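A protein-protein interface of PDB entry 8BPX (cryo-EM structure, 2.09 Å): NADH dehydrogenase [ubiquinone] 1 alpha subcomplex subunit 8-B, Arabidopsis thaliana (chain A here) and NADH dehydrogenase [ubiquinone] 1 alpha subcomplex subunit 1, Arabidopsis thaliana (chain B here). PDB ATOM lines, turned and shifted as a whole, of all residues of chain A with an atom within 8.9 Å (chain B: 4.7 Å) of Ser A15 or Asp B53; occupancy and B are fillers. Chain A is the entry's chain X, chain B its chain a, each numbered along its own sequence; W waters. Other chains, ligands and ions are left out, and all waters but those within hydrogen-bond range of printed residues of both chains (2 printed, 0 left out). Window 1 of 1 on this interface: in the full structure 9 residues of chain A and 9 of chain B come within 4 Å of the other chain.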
ATOM      1  N   ILE A  12      16.722  10.243 -20.719  1.00  0.00           N
ATOM      2  CA  ILE A  12      17.880  10.375 -21.598  1.00  0.00           C
ATOM      3  C   ILE A  12      18.350  11.820 -21.499  1.00  0.00           C
ATOM      4  O   ILE A  12      17.575  12.743 -21.790  1.00  0.00           O
ATOM      5  CB  ILE A  12      17.541   9.982 -23.042  1.00  0.00           C
ATOM      6  CG1 ILE A  12      16.793   8.647 -23.069  1.00  0.00           C
ATOM      7  CG2 ILE A  12      18.803   9.904 -23.887  1.00  0.00           C
ATOM      8  CD1 ILE A  12      17.629   7.469 -22.619  1.00  0.00           C
ATOM      9  N   PRO A  13      19.594  12.066 -21.095  1.00  0.00           N
ATOM     10  CA  PRO A  13      20.069  13.445 -20.891  1.00  0.00           C
ATOM     11  C   PRO A  13      20.384  14.148 -22.206  1.00  0.00           C
ATOM     12  O   PRO A  13      21.521  14.537 -22.484  1.00  0.00           O
ATOM     13  CB  PRO A  13      21.312  13.230 -20.020  1.00  0.00           C
ATOM     14  CG  PRO A  13      21.848  11.925 -20.488  1.00  0.00           C
ATOM     15  CD  PRO A  13      20.658  11.076 -20.850  1.00  0.00           C
ATOM     16  N   THR A  14      19.356  14.317 -23.029  1.00  0.00           N
ATOM     17  CA  THR A  14      19.500  15.008 -24.298  1.00  0.00           C
ATOM     18  C   THR A  14      19.670  16.506 -24.063  1.00  0.00           C
ATOM     19  O   THR A  14      19.590  17.003 -22.937  1.00  0.00           O
ATOM     20  CB  THR A  14      18.291  14.741 -25.190  1.00  0.00           C
ATOM     21  OG1 THR A  14      17.107  15.210 -24.534  1.00  0.00           O
ATOM     22  CG2 THR A  14      18.160  13.259 -25.463  1.00  0.00           C
ATOM     23  N   SER A  15      19.900  17.235 -25.156  1.00  0.00           N
ATOM     24  CA  SER A  15      20.041  18.684 -25.061  1.00  0.00           C
ATOM     25  C   SER A  15      18.767  19.325 -24.528  1.00  0.00           C
ATOM     26  O   SER A  15      18.826  20.290 -23.760  1.00  0.00           O
ATOM     27  CB  SER A  15      20.413  19.263 -26.428  1.00  0.00           C
ATOM     28  OG  SER A  15      19.384  19.057 -27.378  1.00  0.00           O
ATOM     29  N   ALA A  16      17.603  18.807 -24.929  1.00  0.00           N
ATOM     30  CA  ALA A  16      16.342  19.367 -24.453  1.00  0.00           C
ATOM     31  C   ALA A  16      16.198  19.205 -22.944  1.00  0.00           C
ATOM     32  O   ALA A  16      15.849  20.156 -22.239  1.00  0.00           O
ATOM     33  CB  ALA A  16      15.167  18.712 -25.181  1.00  0.00           C
ATOM     34  N   VAL A  17      16.471  18.002 -22.430  1.00  0.00           N
ATOM     35  CA  VAL A  17      16.321  17.753 -20.996  1.00  0.00           C
ATOM     36  C   VAL A  17      17.267  18.641 -20.198  1.00  0.00           C
ATOM     37  O   VAL A  17      16.865  19.301 -19.231  1.00  0.00           O
ATOM     38  CB  VAL A  17      16.552  16.262 -20.687  1.00  0.00           C
ATOM     39  CG1 VAL A  17      16.678  16.048 -19.188  1.00  0.00           C
ATOM     40  CG2 VAL A  17      15.422  15.419 -21.265  1.00  0.00           C
ATOM     41  N   LEU A  18      18.536  18.687 -20.610  1.00  0.00           N
ATOM     42  CA  LEU A  18      19.525  19.479 -19.887  1.00  0.00           C
ATOM     43  C   LEU A  18      19.194  20.965 -19.945  1.00  0.00           C
ATOM     44  O   LEU A  18      19.272  21.664 -18.932  1.00  0.00           O
ATOM     45  CB  LEU A  18      20.920  19.207 -20.446  1.00  0.00           C
ATOM     46  CG  LEU A  18      21.410  17.769 -20.262  1.00  0.00           C
ATOM     47  CD1 LEU A  18      22.686  17.520 -21.049  1.00  0.00           C
ATOM     48  CD2 LEU A  18      21.611  17.467 -18.788  1.00  0.00           C
ATOM     49  N   THR A  19      18.826  21.468 -21.126  1.00  0.00           N
ATOM     50  CA  THR A  19      18.503  22.886 -21.241  1.00  0.00           C
ATOM     51  C   THR A  19      17.281  23.240 -20.405  1.00  0.00           C
ATOM     52  O   THR A  19      17.274  24.262 -19.711  1.00  0.00           O
ATOM     53  CB  THR A  19      18.292  23.273 -22.706  1.00  0.00           C
ATOM     54  OG1 THR A  19      19.354  22.734 -23.502  1.00  0.00           O
ATOM     55  CG2 THR A  19      18.293  24.784 -22.852  1.00  0.00           C
ATOM     56  N   ALA A  20      16.246  22.396 -20.435  1.00  0.00           N
ATOM     57  CA  ALA A  20      15.063  22.658 -19.626  1.00  0.00           C
ATOM     58  C   ALA A  20      15.381  22.624 -18.134  1.00  0.00           C
ATOM     59  O   ALA A  20      14.782  23.377 -17.360  1.00  0.00           O
ATOM     60  CB  ALA A  20      13.961  21.653 -19.960  1.00  0.00           C
ATOM     61  N   SER A  21      16.315  21.773 -17.716  1.00  0.00           N
ATOM     62  CA  SER A  21      16.666  21.654 -16.305  1.00  0.00           C
ATOM     63  C   SER A  21      17.838  22.540 -15.895  1.00  0.00           C
ATOM     64  O   SER A  21      18.274  22.454 -14.745  1.00  0.00           O
ATOM     65  CB  SER A  21      16.996  20.198 -15.968  1.00  0.00           C
ATOM     66  OG  SER A  21      15.882  19.357 -16.198  1.00  0.00           O
ATOM     67  N   ALA A  22      18.354  23.362 -16.814  1.00  0.00           N
ATOM     68  CA  ALA A  22      19.589  24.106 -16.574  1.00  0.00           C
ATOM     69  C   ALA A  22      19.523  24.972 -15.320  1.00  0.00           C
ATOM     70  O   ALA A  22      20.515  25.087 -14.597  1.00  0.00           O
ATOM     71  CB  ALA A  22      19.925  24.958 -17.796  1.00  0.00           C
ATOM     72  N   ILE A  25      19.900  22.787 -12.384  1.00  0.00           N
ATOM     73  CA  ILE A  25      21.264  22.271 -12.369  1.00  0.00           C
ATOM     74  C   ILE A  25      22.221  23.317 -11.813  1.00  0.00           C
ATOM     75  O   ILE A  25      23.086  23.013 -10.983  1.00  0.00           O
ATOM     76  CB  ILE A  25      21.672  21.815 -13.782  1.00  0.00           C
ATOM     77  CG1 ILE A  25      20.876  20.575 -14.194  1.00  0.00           C
ATOM     78  CG2 ILE A  25      23.161  21.540 -13.849  1.00  0.00           C
ATOM     79  CD1 ILE A  25      21.254  20.023 -15.548  1.00  0.00           C
ATOM     80  N   LEU A  64      18.490  15.020 -12.118  1.00  0.00           N
ATOM     81  CA  LEU A  64      17.564  14.691 -13.199  1.00  0.00           C
ATOM     82  C   LEU A  64      16.556  13.643 -12.749  1.00  0.00           C
ATOM     83  O   LEU A  64      15.344  13.799 -12.946  1.00  0.00           O
ATOM     84  CB  LEU A  64      18.340  14.185 -14.417  1.00  0.00           C
ATOM     85  CG  LEU A  64      18.938  15.160 -15.435  1.00  0.00           C
ATOM     86  CD1 LEU A  64      19.053  14.485 -16.788  1.00  0.00           C
ATOM     87  CD2 LEU A  64      18.136  16.435 -15.542  1.00  0.00           C
ATOM     88  N   VAL A  79      10.015  19.604 -21.423  1.00  0.00           N
ATOM     89  CA  VAL A  79      11.061  19.025 -22.259  1.00  0.00           C
ATOM     90  C   VAL A  79      10.575  18.876 -23.695  1.00  0.00           C
ATOM     91  O   VAL A  79      11.318  19.142 -24.646  1.00  0.00           O
ATOM     92  CB  VAL A  79      11.524  17.679 -21.665  1.00  0.00           C
ATOM     93  CG1 VAL A  79      12.318  16.881 -22.681  1.00  0.00           C
ATOM     94  CG2 VAL A  79      12.342  17.911 -20.402  1.00  0.00           C
ATOM     95  N   MET A  82      10.483  22.305 -25.321  1.00  0.00           N
ATOM     96  CA  MET A  82      11.852  22.762 -25.531  1.00  0.00           C
ATOM     97  C   MET A  82      12.495  22.055 -26.717  1.00  0.00           C
ATOM     98  O   MET A  82      13.224  22.677 -27.499  1.00  0.00           O
ATOM     99  CB  MET A  82      12.675  22.536 -24.264  1.00  0.00           C
ATOM    100  CG  MET A  82      12.459  23.590 -23.198  1.00  0.00           C
ATOM    101  SD  MET A  82      13.123  25.191 -23.685  1.00  0.00           S
ATOM    102  CE  MET A  82      14.764  25.064 -22.992  1.00  0.00           C
ATOM    103  N   TYR A  83      12.250  20.752 -26.861  1.00  0.00           N
ATOM    104  CA  TYR A  83      12.771  20.043 -28.023  1.00  0.00           C
ATOM    105  C   TYR A  83      12.091  20.520 -29.300  1.00  0.00           C
ATOM    106  O   TYR A  83      12.738  20.655 -30.343  1.00  0.00           O
ATOM    107  CB  TYR A  83      12.595  18.533 -27.854  1.00  0.00           C
ATOM    108  CG  TYR A  83      12.770  17.774 -29.150  1.00  0.00           C
ATOM    109  CD1 TYR A  83      14.027  17.356 -29.559  1.00  0.00           C
ATOM    110  CD2 TYR A  83      11.682  17.484 -29.967  1.00  0.00           C
ATOM    111  CE1 TYR A  83      14.201  16.676 -30.745  1.00  0.00           C
ATOM    112  CE2 TYR A  83      11.846  16.808 -31.153  1.00  0.00           C
ATOM    113  CZ  TYR A  83      13.108  16.405 -31.538  1.00  0.00           C
ATOM    114  OH  TYR A  83      13.274  15.726 -32.719  1.00  0.00           O
ATOM    115  N   THR A  86      13.597  23.796 -30.269  1.00  0.00           N
ATOM    116  CA  THR A  86      15.057  23.781 -30.183  1.00  0.00           C
ATOM    117  C   THR A  86      15.548  24.689 -29.053  1.00  0.00           C
ATOM    118  O   THR A  86      16.346  25.609 -29.253  1.00  0.00           O
ATOM    119  CB  THR A  86      15.695  24.155 -31.525  1.00  0.00           C
ATOM    120  OG1 THR A  86      15.028  23.455 -32.579  1.00  0.00           O
ATOM    121  CG2 THR A  86      17.169  23.760 -31.552  1.00  0.00           C
ATOM    122  N   ASN A  87      15.021  24.441 -27.855  1.00  0.00           N
ATOM    123  CA  ASN A  87      15.510  25.038 -26.612  1.00  0.00           C
ATOM    124  C   ASN A  87      15.371  26.561 -26.587  1.00  0.00           C
ATOM    125  O   ASN A  87      16.178  27.251 -25.964  1.00  0.00           O
ATOM    126  CB  ASN A  87      16.963  24.633 -26.346  1.00  0.00           C
ATOM    127  CG  ASN A  87      17.147  23.133 -26.326  1.00  0.00           C
ATOM    128  OD1 ASN A  87      16.337  22.407 -25.753  1.00  0.00           O
ATOM    129  ND2 ASN A  87      18.210  22.656 -26.960  1.00  0.00           N
ATOM    130  N   GLU A  88      14.341  27.101 -27.238  1.00  0.00           N
ATOM    131  CA  GLU A  88      14.072  28.536 -27.211  1.00  0.00           C
ATOM    132  C   GLU A  88      13.140  28.833 -26.040  1.00  0.00           C
ATOM    133  O   GLU A  88      11.948  28.514 -26.092  1.00  0.00           O
ATOM    134  CB  GLU A  88      13.466  29.004 -28.531  1.00  0.00           C
ATOM    135  CG  GLU A  88      13.737  30.461 -28.847  1.00  0.00           C
ATOM    136  CD  GLU A  88      15.211  30.813 -28.731  1.00  0.00           C
ATOM    137  OE1 GLU A  88      15.989  30.414 -29.619  1.00  0.00           O
ATOM    138  OE2 GLU A  88      15.588  31.485 -27.748  1.00  0.00           O
ATOM    139  N   PHE A  89      13.684  29.464 -24.994  1.00  0.00           N
ATOM    140  CA  PHE A  89      12.933  29.651 -23.756  1.00  0.00           C
ATOM    141  C   PHE A  89      11.659  30.460 -23.979  1.00  0.00           C
ATOM    142  O   PHE A  89      10.627  30.184 -23.360  1.00  0.00           O
ATOM    143  CB  PHE A  89      13.813  30.330 -22.705  1.00  0.00           C
ATOM    144  CG  PHE A  89      14.902  29.448 -22.159  1.00  0.00           C
ATOM    145  CD1 PHE A  89      14.602  28.404 -21.299  1.00  0.00           C
ATOM    146  CD2 PHE A  89      16.223  29.666 -22.504  1.00  0.00           C
ATOM    147  CE1 PHE A  89      15.600  27.592 -20.792  1.00  0.00           C
ATOM    148  CE2 PHE A  89      17.227  28.854 -21.999  1.00  0.00           C
ATOM    149  CZ  PHE A  89      16.910  27.815 -21.144  1.00  0.00           C
ATOM    150  N   MET B  49      25.141  20.436 -30.096  1.00  0.00           N
ATOM    151  CA  MET B  49      24.095  19.756 -29.341  1.00  0.00           C
ATOM    152  C   MET B  49      23.409  18.687 -30.179  1.00  0.00           C
ATOM    153  O   MET B  49      23.191  17.569 -29.709  1.00  0.00           O
ATOM    154  CB  MET B  49      23.070  20.768 -28.824  1.00  0.00           C
ATOM    155  CG  MET B  49      23.452  21.640 -27.609  1.00  0.00           C
ATOM    156  SD  MET B  49      24.399  20.931 -26.230  1.00  0.00           S
ATOM    157  CE  MET B  49      26.065  20.803 -26.869  1.00  0.00           C
ATOM    158  N   GLU B  50      23.051  19.014 -31.422  1.00  0.00           N
ATOM    159  CA  GLU B  50      22.399  18.031 -32.284  1.00  0.00           C
ATOM    160  C   GLU B  50      23.321  16.856 -32.600  1.00  0.00           C
ATOM    161  O   GLU B  50      22.891  15.692 -32.561  1.00  0.00           O
ATOM    162  CB  GLU B  50      21.902  18.705 -33.564  1.00  0.00           C
ATOM    163  CG  GLU B  50      20.773  19.702 -33.335  1.00  0.00           C
ATOM    164  CD  GLU B  50      20.333  20.422 -34.596  1.00  0.00           C
ATOM    165  OE1 GLU B  50      21.031  20.288 -35.627  1.00  0.00           O
ATOM    166  OE2 GLU B  50      19.317  21.145 -34.556  1.00  0.00           O
ATOM    167  N   ARG B  51      24.593  17.133 -32.897  1.00  0.00           N
ATOM    168  CA  ARG B  51      25.519  16.044 -33.198  1.00  0.00           C
ATOM    169  C   ARG B  51      25.720  15.134 -31.989  1.00  0.00           C
ATOM    170  O   ARG B  51      25.751  13.907 -32.133  1.00  0.00           O
ATOM    171  CB  ARG B  51      26.860  16.595 -33.686  1.00  0.00           C
ATOM    172  CG  ARG B  51      26.863  16.985 -35.155  1.00  0.00           C
ATOM    173  CD  ARG B  51      27.797  18.151 -35.415  1.00  0.00           C
ATOM    174  NE  ARG B  51      27.573  18.759 -36.720  1.00  0.00           N
ATOM    175  CZ  ARG B  51      28.519  19.335 -37.450  1.00  0.00           C
ATOM    176  NH1 ARG B  51      29.777  19.373 -37.045  1.00  0.00           N
ATOM    177  NH2 ARG B  51      28.190  19.893 -38.610  1.00  0.00           N
ATOM    178  N   ARG B  52      25.856  15.709 -30.792  1.00  0.00           N
ATOM    179  CA  ARG B  52      26.010  14.881 -29.599  1.00  0.00           C
ATOM    180  C   ARG B  52      24.714  14.156 -29.247  1.00  0.00           C
ATOM    181  O   ARG B  52      24.750  13.025 -28.741  1.00  0.00           O
ATOM    182  CB  ARG B  52      26.496  15.747 -28.437  1.00  0.00           C
ATOM    183  CG  ARG B  52      26.531  15.061 -27.094  1.00  0.00           C
ATOM    184  CD  ARG B  52      25.979  15.971 -26.020  1.00  0.00           C
ATOM    185  NE  ARG B  52      25.756  15.277 -24.758  1.00  0.00           N
ATOM    186  CZ  ARG B  52      24.563  15.090 -24.212  1.00  0.00           C
ATOM    187  NH1 ARG B  52      23.458  15.515 -24.801  1.00  0.00           N
ATOM    188  NH2 ARG B  52      24.476  14.456 -23.046  1.00  0.00           N
ATOM    189  N   ASP B  53      23.564  14.772 -29.537  1.00  0.00           N
ATOM    190  CA  ASP B  53      22.282  14.152 -29.229  1.00  0.00           C
ATOM    191  C   ASP B  53      22.013  12.959 -30.126  1.00  0.00           C
ATOM    192  O   ASP B  53      21.343  12.013 -29.701  1.00  0.00           O
ATOM    193  CB  ASP B  53      21.154  15.175 -29.359  1.00  0.00           C
ATOM    194  CG  ASP B  53      20.766  15.780 -28.028  1.00  0.00           C
ATOM    195  OD1 ASP B  53      21.599  15.748 -27.100  1.00  0.00           O
ATOM    196  OD2 ASP B  53      19.633  16.291 -27.908  1.00  0.00           O
ATOM    197  N   LYS B  54      22.512  12.988 -31.366  1.00  0.00           N
ATOM    198  CA  LYS B  54      22.416  11.800 -32.209  1.00  0.00           C
ATOM    199  C   LYS B  54      23.012  10.589 -31.502  1.00  0.00           C
ATOM    200  O   LYS B  54      22.395   9.521 -31.446  1.00  0.00           O
ATOM    201  CB  LYS B  54      23.119  12.023 -33.551  1.00  0.00           C
ATOM    202  CG  LYS B  54      22.558  13.140 -34.405  1.00  0.00           C
ATOM    203  CD  LYS B  54      23.451  13.381 -35.610  1.00  0.00           C
ATOM    204  CE  LYS B  54      23.060  14.641 -36.361  1.00  0.00           C
ATOM    205  NZ  LYS B  54      23.998  14.919 -37.485  1.00  0.00           N
ATOM    206  N   LYS B  55      24.215  10.748 -30.943  1.00  0.00           N
ATOM    207  CA  LYS B  55      24.837   9.663 -30.190  1.00  0.00           C
ATOM    208  C   LYS B  55      24.019   9.313 -28.953  1.00  0.00           C
ATOM    209  O   LYS B  55      23.653   8.149 -28.747  1.00  0.00           O
ATOM    210  CB  LYS B  55      26.264  10.043 -29.797  1.00  0.00           C
ATOM    211  CG  LYS B  55      27.111  10.617 -30.923  1.00  0.00           C
ATOM    212  CD  LYS B  55      27.025   9.776 -32.185  1.00  0.00           C
ATOM    213  CE  LYS B  55      27.701  10.476 -33.356  1.00  0.00           C
ATOM    214  NZ  LYS B  55      28.202   9.506 -34.369  1.00  0.00           N
ATOM    215  N   VAL B  56      23.693  10.316 -28.132  1.00  0.00           N
ATOM    216  CA  VAL B  56      23.002  10.055 -26.869  1.00  0.00           C
ATOM    217  C   VAL B  56      21.649   9.377 -27.083  1.00  0.00           C
ATOM    218  O   VAL B  56      21.161   8.676 -26.191  1.00  0.00           O
ATOM    219  CB  VAL B  56      22.858  11.366 -26.063  1.00  0.00           C
ATOM    220  CG1 VAL B  56      22.240  11.102 -24.705  1.00  0.00           C
ATOM    221  CG2 VAL B  56      24.216  12.015 -25.873  1.00  0.00           C
ATOM    222  N   VAL B  57      21.043   9.536 -28.257  1.00  0.00           N
ATOM    223  CA  VAL B  57      19.781   8.869 -28.550  1.00  0.00           C
ATOM    224  C   VAL B  57      20.040   7.493 -29.150  1.00  0.00           C
ATOM    225  O   VAL B  57      19.598   6.477 -28.603  1.00  0.00           O
ATOM    226  CB  VAL B  57      18.907   9.722 -29.489  1.00  0.00           C
ATOM    227  CG1 VAL B  57      17.722   8.911 -29.994  1.00  0.00           C
ATOM    228  CG2 VAL B  57      18.430  10.973 -28.771  1.00  0.00           C
ATOM    229  N   GLU B  58      20.755   7.447 -30.280  1.00  0.00           N
ATOM    230  CA  GLU B  58      20.887   6.204 -31.034  1.00  0.00           C
ATOM    231  C   GLU B  58      21.624   5.136 -30.234  1.00  0.00           C
ATOM    232  O   GLU B  58      21.301   3.945 -30.332  1.00  0.00           O
ATOM    233  CB  GLU B  58      21.597   6.475 -32.361  1.00  0.00           C
ATOM    234  CG  GLU B  58      21.737   5.260 -33.262  1.00  0.00           C
ATOM    235  CD  GLU B  58      22.318   5.607 -34.619  1.00  0.00           C
ATOM    236  OE1 GLU B  58      23.052   6.613 -34.712  1.00  0.00           O
ATOM    237  OE2 GLU B  58      22.039   4.876 -35.592  1.00  0.00           O
HETATM  238  O   HOH W   1      17.226  17.336 -27.246  1.00  0.00           O
HETATM  239  O   HOH W   2      19.883  19.122 -30.789  1.00  0.00           O
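OG of Ser A15 sits at hydrogen-bond distance from OD2 of Asp B53.
NH2 of Arg B52 sits at hydrogen-bond distance from O of Pro A13.
The backbone carbonyl oxygen of Ser A15 is in hydrogen-bond range of the side-chain hydroxyl of Thr A19, 2.5 Å away.
The guanidinium group of Arg B52 lies within salt-bridge range of the side-chain carboxylate of Asp B53, 3.0 Å away.
Among the printed residues, pairs that only touch across the chains: Ile A12 with Val B56, Thr A14 with Arg B52, Thr A14 with Asp B53, Ser A15 with Met B49 and Ser A15 with Arg B52.
Ser A15 touches just these residues of chain B: Met B49, Arg B52 and Asp B53.
Asp B53 touches just these residues of chain A: Thr A14 and Ser A15.
Printed residues of chain B within 4 Å of Thr A14: Arg B52 (3.98 Å) and Asp B53 (3.4 Å).
Of the printed residues of chain A, Met B49 touches Ser A15.
The nearest printed residue of chain B that does not touch Ser A15 is Glu B50 (5.5 Å).
The nearest printed residue of chain B that does not touch Pro A13 is Val B56 (4.2 Å).
Hydrophobic or aromatic side chains of chain B within 4 Å of the printed part of chain A: Met B49 and Val B56.
Along chain B the printed residues that touch a printed residue of chain A span positions 49 to 56.
Of the 20 printed residues of chain A, 4 touch a printed residue of chain B.
Printed residues of chain A that touch a printed residue of chain B: Ile A12, Pro A13, Thr A14 and Ser A15.
Hydrophobic or aromatic side chains of chain A within 4 Å of the printed part of chain B: Ile A12.
Among the printed residues, 7 pairs touch across the chains.
Among the printed residues, no Asp or Glu carboxylate lies within 4 Å of a Lys or Arg side-chain nitrogen of the other chain.
Water W1 lies within hydrogen-bond range of the side-chain carboxylate of Asp B53 (2.7 Å), the side-chain hydroxyl of Ser A15 (2.8 Å), the backbone NH of Ala A16 (2.8 Å) and the side-chain hydroxyl of Thr A14 (3.4 Å).
Water W2 lies within hydrogen-bond range of N of Glu B50 (3.2 Å) and OG of Ser A15 (3.4 Å).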
